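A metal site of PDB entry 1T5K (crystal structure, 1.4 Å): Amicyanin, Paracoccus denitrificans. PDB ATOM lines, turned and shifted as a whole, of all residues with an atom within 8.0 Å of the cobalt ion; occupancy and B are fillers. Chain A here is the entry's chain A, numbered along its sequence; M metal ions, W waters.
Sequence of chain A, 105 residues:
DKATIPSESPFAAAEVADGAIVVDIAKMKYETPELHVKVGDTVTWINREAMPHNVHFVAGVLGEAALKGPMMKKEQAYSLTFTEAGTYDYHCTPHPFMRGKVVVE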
ATOM      1  N   ILE A  25      -9.976 -11.604  -5.795  1.00  0.00           N
ATOM      2  CA  ILE A  25     -10.574 -12.573  -6.710  1.00  0.00           C
ATOM      3  C   ILE A  25      -9.482 -12.950  -7.695  1.00  0.00           C
ATOM      4  O   ILE A  25      -8.950 -12.118  -8.424  1.00  0.00           O
ATOM      5  CB  ILE A  25     -11.801 -12.003  -7.462  1.00  0.00           C
ATOM      6  CG1 ILE A  25     -12.750 -11.280  -6.522  1.00  0.00           C
ATOM      7  CG2 ILE A  25     -12.515 -13.138  -8.172  1.00  0.00           C
ATOM      8  CD1 ILE A  25     -13.895 -10.527  -7.220  1.00  0.00           C
ATOM      9  N   MET A  28     -10.143 -17.936 -10.442  1.00  0.00           N
ATOM     10  CA  MET A  28     -11.560 -18.290 -10.463  1.00  0.00           C
ATOM     11  C   MET A  28     -12.117 -18.588  -9.085  1.00  0.00           C
ATOM     12  O   MET A  28     -12.968 -19.493  -8.932  1.00  0.00           O
ATOM     13  CB  MET A  28     -11.839 -19.428 -11.443  1.00  0.00           C
ATOM     14  CG  MET A  28     -11.542 -19.056 -12.906  1.00  0.00           C
ATOM     15  SD  MET A  28     -12.617 -17.859 -13.655  1.00  0.00           S
ATOM     16  CE  MET A  28     -14.174 -18.598 -13.497  1.00  0.00           C
ATOM     17  N   LYS A  29     -11.698 -17.808  -8.103  1.00  0.00           N
ATOM     18  CA  LYS A  29     -12.190 -17.994  -6.769  1.00  0.00           C
ATOM     19  C   LYS A  29     -12.065 -16.721  -5.958  1.00  0.00           C
ATOM     20  O   LYS A  29     -11.295 -15.838  -6.236  1.00  0.00           O
ATOM     21  CB  LYS A  29     -11.589 -19.199  -6.069  1.00  0.00           C
ATOM     22  CG  LYS A  29     -10.186 -19.207  -5.788  1.00  0.00           C
ATOM     23  CD  LYS A  29      -9.754 -20.716  -5.428  1.00  0.00           C
ATOM     24  CE  LYS A  29     -10.071 -21.760  -6.577  1.00  0.00           C
ATOM     25  NZ  LYS A  29     -10.777 -23.130  -6.308  1.00  0.00           N
ATOM     26  N   TYR A  30     -12.916 -16.673  -4.949  1.00  0.00           N
ATOM     27  CA  TYR A  30     -12.822 -15.634  -3.931  1.00  0.00           C
ATOM     28  C   TYR A  30     -11.734 -16.120  -2.971  1.00  0.00           C
ATOM     29  O   TYR A  30     -11.902 -17.152  -2.343  1.00  0.00           O
ATOM     30  CB  TYR A  30     -14.184 -15.438  -3.247  1.00  0.00           C
ATOM     31  CG  TYR A  30     -15.268 -14.900  -4.164  1.00  0.00           C
ATOM     32  CD1 TYR A  30     -15.217 -13.609  -4.690  1.00  0.00           C
ATOM     33  CD2 TYR A  30     -16.349 -15.681  -4.519  1.00  0.00           C
ATOM     34  CE1 TYR A  30     -16.192 -13.173  -5.560  1.00  0.00           C
ATOM     35  CE2 TYR A  30     -17.321 -15.234  -5.342  1.00  0.00           C
ATOM     36  CZ  TYR A  30     -17.217 -14.004  -5.868  1.00  0.00           C
ATOM     37  OH  TYR A  30     -18.275 -13.578  -6.670  1.00  0.00           O
ATOM     38  N   ASN A  47     -10.575  -7.605  -8.191  1.00  0.00           N
ATOM     39  CA  ASN A  47     -10.374  -8.623  -9.209  1.00  0.00           C
ATOM     40  C   ASN A  47      -8.974  -8.555  -9.753  1.00  0.00           C
ATOM     41  O   ASN A  47      -8.564  -7.494 -10.226  1.00  0.00           O
ATOM     42  CB  ASN A  47     -11.420  -8.508 -10.324  1.00  0.00           C
ATOM     43  CG  ASN A  47     -11.314  -9.627 -11.324  1.00  0.00           C
ATOM     44  OD1 ASN A  47     -10.639 -10.661 -11.067  1.00  0.00           O
ATOM     45  ND2 ASN A  47     -11.909  -9.449 -12.476  1.00  0.00           N
ATOM     46  N   GLU A  49      -7.730 -10.808 -12.025  1.00  0.00           N
ATOM     47  CA  GLU A  49      -7.527 -11.509 -13.280  1.00  0.00           C
ATOM     48  C   GLU A  49      -8.257 -10.890 -14.444  1.00  0.00           C
ATOM     49  O   GLU A  49      -9.102 -10.027 -14.276  1.00  0.00           O
ATOM     50  CB  GLU A  49      -7.767 -13.036 -13.155  1.00  0.00           C
ATOM     51  CG  GLU A  49      -9.114 -13.445 -12.564  1.00  0.00           C
ATOM     52  CD  GLU A  49      -9.374 -14.981 -12.428  1.00  0.00           C
ATOM     53  OE1 GLU A  49      -8.614 -15.829 -12.947  1.00  0.00           O
ATOM     54  OE2 GLU A  49     -10.395 -15.371 -11.809  1.00  0.00           O
ATOM     55  N   MET A  51     -10.307 -12.233 -16.563  1.00  0.00           N
ATOM     56  CA  MET A  51     -11.725 -12.546 -16.579  1.00  0.00           C
ATOM     57  C   MET A  51     -12.496 -11.637 -15.592  1.00  0.00           C
ATOM     58  O   MET A  51     -12.169 -11.662 -14.396  1.00  0.00           O
ATOM     59  CB  MET A  51     -11.890 -14.013 -16.157  1.00  0.00           C
ATOM     60  CG  MET A  51     -13.329 -14.447 -15.971  1.00  0.00           C
ATOM     61  SD  MET A  51     -14.308 -14.276 -17.464  1.00  0.00           S
ATOM     62  CE  MET A  51     -13.637 -15.614 -18.495  1.00  0.00           C
ATOM     63  N   PRO A  52     -13.458 -10.832 -16.051  1.00  0.00           N
ATOM     64  CA  PRO A  52     -14.237 -10.022 -15.125  1.00  0.00           C
ATOM     65  C   PRO A  52     -15.073 -10.910 -14.211  1.00  0.00           C
ATOM     66  O   PRO A  52     -15.490 -12.015 -14.578  1.00  0.00           O
ATOM     67  CB  PRO A  52     -15.094  -9.154 -16.033  1.00  0.00           C
ATOM     68  CG  PRO A  52     -14.394  -9.156 -17.288  1.00  0.00           C
ATOM     69  CD  PRO A  52     -13.822 -10.553 -17.444  1.00  0.00           C
ATOM     70  N   HIS A  53     -15.367 -10.389 -13.012  1.00  0.00           N
ATOM     71  CA  HIS A  53     -16.206 -11.065 -12.020  1.00  0.00           C
ATOM     72  C   HIS A  53     -16.955 -10.007 -11.221  1.00  0.00           C
ATOM     73  O   HIS A  53     -16.509  -8.878 -11.154  1.00  0.00           O
ATOM     74  CB  HIS A  53     -15.346 -11.839 -11.020  1.00  0.00           C
ATOM     75  CG  HIS A  53     -14.570 -12.979 -11.597  1.00  0.00           C
ATOM     76  ND1 HIS A  53     -15.191 -14.135 -12.090  1.00  0.00           N
ATOM     77  CD2 HIS A  53     -13.230 -13.182 -11.622  1.00  0.00           C
ATOM     78  CE1 HIS A  53     -14.205 -14.967 -12.430  1.00  0.00           C
ATOM     79  NE2 HIS A  53     -13.026 -14.422 -12.173  1.00  0.00           N
ATOM     80  N   ASN A  54     -18.032 -10.400 -10.540  1.00  0.00           N
ATOM     81  CA  ASN A  54     -18.764  -9.506  -9.614  1.00  0.00           C
ATOM     82  C   ASN A  54     -19.013 -10.242  -8.336  1.00  0.00           C
ATOM     83  O   ASN A  54     -18.457 -11.329  -8.125  1.00  0.00           O
ATOM     84  CB  ASN A  54     -20.084  -9.024 -10.254  1.00  0.00           C
ATOM     85  CG  ASN A  54     -21.139 -10.102 -10.343  1.00  0.00           C
ATOM     86  OD1 ASN A  54     -20.866 -11.323 -10.241  1.00  0.00           O
ATOM     87  ND2 ASN A  54     -22.371  -9.669 -10.520  1.00  0.00           N
ATOM     88  N   VAL A  55     -19.814  -9.627  -7.454  1.00  0.00           N
ATOM     89  CA  VAL A  55     -20.355 -10.316  -6.305  1.00  0.00           C
ATOM     90  C   VAL A  55     -21.862 -10.132  -6.394  1.00  0.00           C
ATOM     91  O   VAL A  55     -22.301  -9.068  -6.852  1.00  0.00           O
ATOM     92  CB  VAL A  55     -19.840  -9.796  -4.947  1.00  0.00           C
ATOM     93  CG1 VAL A  55     -18.355 -10.137  -4.785  1.00  0.00           C
ATOM     94  CG2 VAL A  55     -20.069  -8.335  -4.795  1.00  0.00           C
ATOM     95  N   MET A  71     -19.654  -5.719 -12.791  1.00  0.00           N
ATOM     96  CA  MET A  71     -18.478  -6.506 -13.162  1.00  0.00           C
ATOM     97  C   MET A  71     -17.219  -5.690 -12.935  1.00  0.00           C
ATOM     98  O   MET A  71     -17.079  -4.566 -13.432  1.00  0.00           O
ATOM     99  CB  MET A  71     -18.553  -6.950 -14.617  1.00  0.00           C
ATOM    100  CG  MET A  71     -19.444  -8.147 -14.826  1.00  0.00           C
ATOM    101  SD  MET A  71     -18.723  -9.622 -14.126  1.00  0.00           S
ATOM    102  CE  MET A  71     -20.187 -10.706 -13.933  1.00  0.00           C
ATOM    103  N   MET A  72     -16.287  -6.286 -12.208  1.00  0.00           N
ATOM    104  CA  MET A  72     -14.967  -5.717 -11.988  1.00  0.00           C
ATOM    105  C   MET A  72     -14.042  -6.292 -13.072  1.00  0.00           C
ATOM    106  O   MET A  72     -13.909  -7.508 -13.170  1.00  0.00           O
ATOM    107  CB  MET A  72     -14.427  -6.129 -10.606  1.00  0.00           C
ATOM    108  CG  MET A  72     -15.069  -5.421  -9.459  1.00  0.00           C
ATOM    109  SD  MET A  72     -14.628  -6.239  -7.879  1.00  0.00           S
ATOM    110  CE  MET A  72     -15.942  -7.493  -7.898  1.00  0.00           C
ATOM    111  N   HIS A  91     -22.094 -15.009  -4.652  1.00  0.00           N
ATOM    112  CA  HIS A  91     -21.524 -15.766  -5.752  1.00  0.00           C
ATOM    113  C   HIS A  91     -21.267 -14.814  -6.877  1.00  0.00           C
ATOM    114  O   HIS A  91     -21.579 -13.632  -6.810  1.00  0.00           O
ATOM    115  CB  HIS A  91     -22.424 -16.933  -6.201  1.00  0.00           C
ATOM    116  CG  HIS A  91     -23.699 -16.505  -6.869  1.00  0.00           C
ATOM    117  ND1 HIS A  91     -24.836 -16.144  -6.171  1.00  0.00           N
ATOM    118  CD2 HIS A  91     -23.991 -16.359  -8.181  1.00  0.00           C
ATOM    119  CE1 HIS A  91     -25.778 -15.806  -7.047  1.00  0.00           C
ATOM    120  NE2 HIS A  91     -25.307 -15.940  -8.268  1.00  0.00           N
ATOM    121  N   CYS A  92     -20.637 -15.307  -7.950  1.00  0.00           N
ATOM    122  CA  CYS A  92     -20.365 -14.500  -9.139  1.00  0.00           C
ATOM    123  C   CYS A  92     -21.471 -14.824 -10.129  1.00  0.00           C
ATOM    124  O   CYS A  92     -21.697 -16.010 -10.415  1.00  0.00           O
ATOM    125  CB  CYS A  92     -19.011 -14.843  -9.707  1.00  0.00           C
ATOM    126  SG  CYS A  92     -18.656 -13.943 -11.264  1.00  0.00           S
ATOM    127  N   THR A  93     -22.173 -13.805 -10.642  1.00  0.00           N
ATOM    128  CA  THR A  93     -23.367 -14.041 -11.430  1.00  0.00           C
ATOM    129  C   THR A  93     -23.218 -15.096 -12.526  1.00  0.00           C
ATOM    130  O   THR A  93     -24.032 -16.019 -12.572  1.00  0.00           O
ATOM    131  CB  THR A  93     -23.893 -12.723 -11.987  1.00  0.00           C
ATOM    132  OG1 THR A  93     -24.249 -11.837 -10.895  1.00  0.00           O
ATOM    133  CG2 THR A  93     -25.161 -12.945 -12.779  1.00  0.00           C
ATOM    134  N   PRO A  94     -22.301 -14.930 -13.476  1.00  0.00           N
ATOM    135  CA  PRO A  94     -22.173 -15.948 -14.534  1.00  0.00           C
ATOM    136  C   PRO A  94     -21.317 -17.143 -14.106  1.00  0.00           C
ATOM    137  O   PRO A  94     -21.228 -18.111 -14.871  1.00  0.00           O
ATOM    138  CB  PRO A  94     -21.472 -15.206 -15.627  1.00  0.00           C
ATOM    139  CG  PRO A  94     -20.599 -14.244 -14.918  1.00  0.00           C
ATOM    140  CD  PRO A  94     -21.388 -13.800 -13.719  1.00  0.00           C
ATOM    141  N   HIS A  95     -20.735 -17.111 -12.904  1.00  0.00           N
ATOM    142  CA  HIS A  95     -19.943 -18.237 -12.401  1.00  0.00           C
ATOM    143  C   HIS A  95     -20.456 -18.593 -11.028  1.00  0.00           C
ATOM    144  O   HIS A  95     -19.763 -18.391 -10.044  1.00  0.00           O
ATOM    145  CB  HIS A  95     -18.474 -17.850 -12.235  1.00  0.00           C
ATOM    146  CG  HIS A  95     -17.825 -17.445 -13.507  1.00  0.00           C
ATOM    147  ND1 HIS A  95     -17.103 -16.272 -13.641  1.00  0.00           N
ATOM    148  CD2 HIS A  95     -17.818 -18.072 -14.699  1.00  0.00           C
ATOM    149  CE1 HIS A  95     -16.685 -16.222 -14.905  1.00  0.00           C
ATOM    150  NE2 HIS A  95     -17.101 -17.289 -15.551  1.00  0.00           N
ATOM    151  N   PRO A  96     -21.681 -19.097 -10.940  1.00  0.00           N
ATOM    152  CA  PRO A  96     -22.296 -19.387  -9.649  1.00  0.00           C
ATOM    153  C   PRO A  96     -21.592 -20.501  -8.827  1.00  0.00           C
ATOM    154  O   PRO A  96     -21.869 -20.675  -7.639  1.00  0.00           O
ATOM    155  CB  PRO A  96     -23.757 -19.725 -10.010  1.00  0.00           C
ATOM    156  CG  PRO A  96     -23.656 -20.255 -11.404  1.00  0.00           C
ATOM    157  CD  PRO A  96     -22.599 -19.406 -12.067  1.00  0.00           C
ATOM    158  N   PHE A  97     -20.655 -21.193  -9.451  1.00  0.00           N
ATOM    159  CA  PHE A  97     -19.807 -22.160  -8.763  1.00  0.00           C
ATOM    160  C   PHE A  97     -18.771 -21.463  -7.861  1.00  0.00           C
ATOM    161  O   PHE A  97     -18.116 -22.110  -7.047  1.00  0.00           O
ATOM    162  CB  PHE A  97     -19.128 -23.123  -9.760  1.00  0.00           C
ATOM    163  CG  PHE A  97     -18.407 -22.446 -10.861  1.00  0.00           C
ATOM    164  CD1 PHE A  97     -17.109 -22.021 -10.679  1.00  0.00           C
ATOM    165  CD2 PHE A  97     -18.995 -22.277 -12.078  1.00  0.00           C
ATOM    166  CE1 PHE A  97     -16.429 -21.398 -11.729  1.00  0.00           C
ATOM    167  CE2 PHE A  97     -18.323 -21.674 -13.122  1.00  0.00           C
ATOM    168  CZ  PHE A  97     -17.043 -21.222 -12.959  1.00  0.00           C
ATOM    169  N   MET A  98     -18.566 -20.153  -8.062  1.00  0.00           N
ATOM    170  CA  MET A  98     -17.702 -19.300  -7.212  1.00  0.00           C
ATOM    171  C   MET A  98     -18.545 -18.720  -6.128  1.00  0.00           C
ATOM    172  O   MET A  98     -19.410 -17.888  -6.396  1.00  0.00           O
ATOM    173  CB  MET A  98     -17.103 -18.117  -7.946  1.00  0.00           C
ATOM    174  CG  MET A  98     -16.155 -18.484  -9.052  1.00  0.00           C
ATOM    175  SD  MET A  98     -15.631 -17.029 -10.081  1.00  0.00           S
ATOM    176  CE  MET A  98     -14.852 -16.016  -8.928  1.00  0.00           C
HETATM  177 CO    CO M   1     -17.124 -14.621 -12.628  1.00  0.00          CO
HETATM  178  O   HOH W   1     -17.811 -13.244 -14.391  1.00  0.00           O
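SD of Met 28 lies close to NE2 of His 53 (3.8 Å). The side-chain amide oxygen (OD1) of Asn 54 sits close to the side-chain sulfur (SG) of Cys 92, at 3.6 Å. A ring nitrogen (NE2) of His 53 sits at hydrogen-bond distance from the side-chain carboxylate (OE2) of Glu 49, 2.8 Å away. SD of Met 98 lies close to ND1 of His 53 (3.6 Å). O of His 53 is in hydrogen-bond range of N of Met 72, at 2.8 Å. The backbone carbonyl oxygen (O) of Met 98 sits at hydrogen-bond distance from the backbone NH (N) of Cys 92 (3.3 Å). The side-chain hydroxyl (OH) of Tyr 30 lies within hydrogen-bond range of the backbone NH (N) of Cys 92, at 3.2 Å. The side-chain sulfur of Met 71 sits close to the backbone NH of His 53 (3.6 Å).
Pro 52 touches the cobalt ion. Met 98 touches the cobalt ion (SD to CO, 3.8 Å). Within 4 Å of the cobalt ion: Pro 52, His 53, Cys 92, His 95 and Met 98.
The cobalt ion is bound by ND1 of His 95, ND1 of His 53, SG of Cys 92 and water W1.
Water W1 lies within hydrogen-bond range of O of Pro 52 and SD of Met 71.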
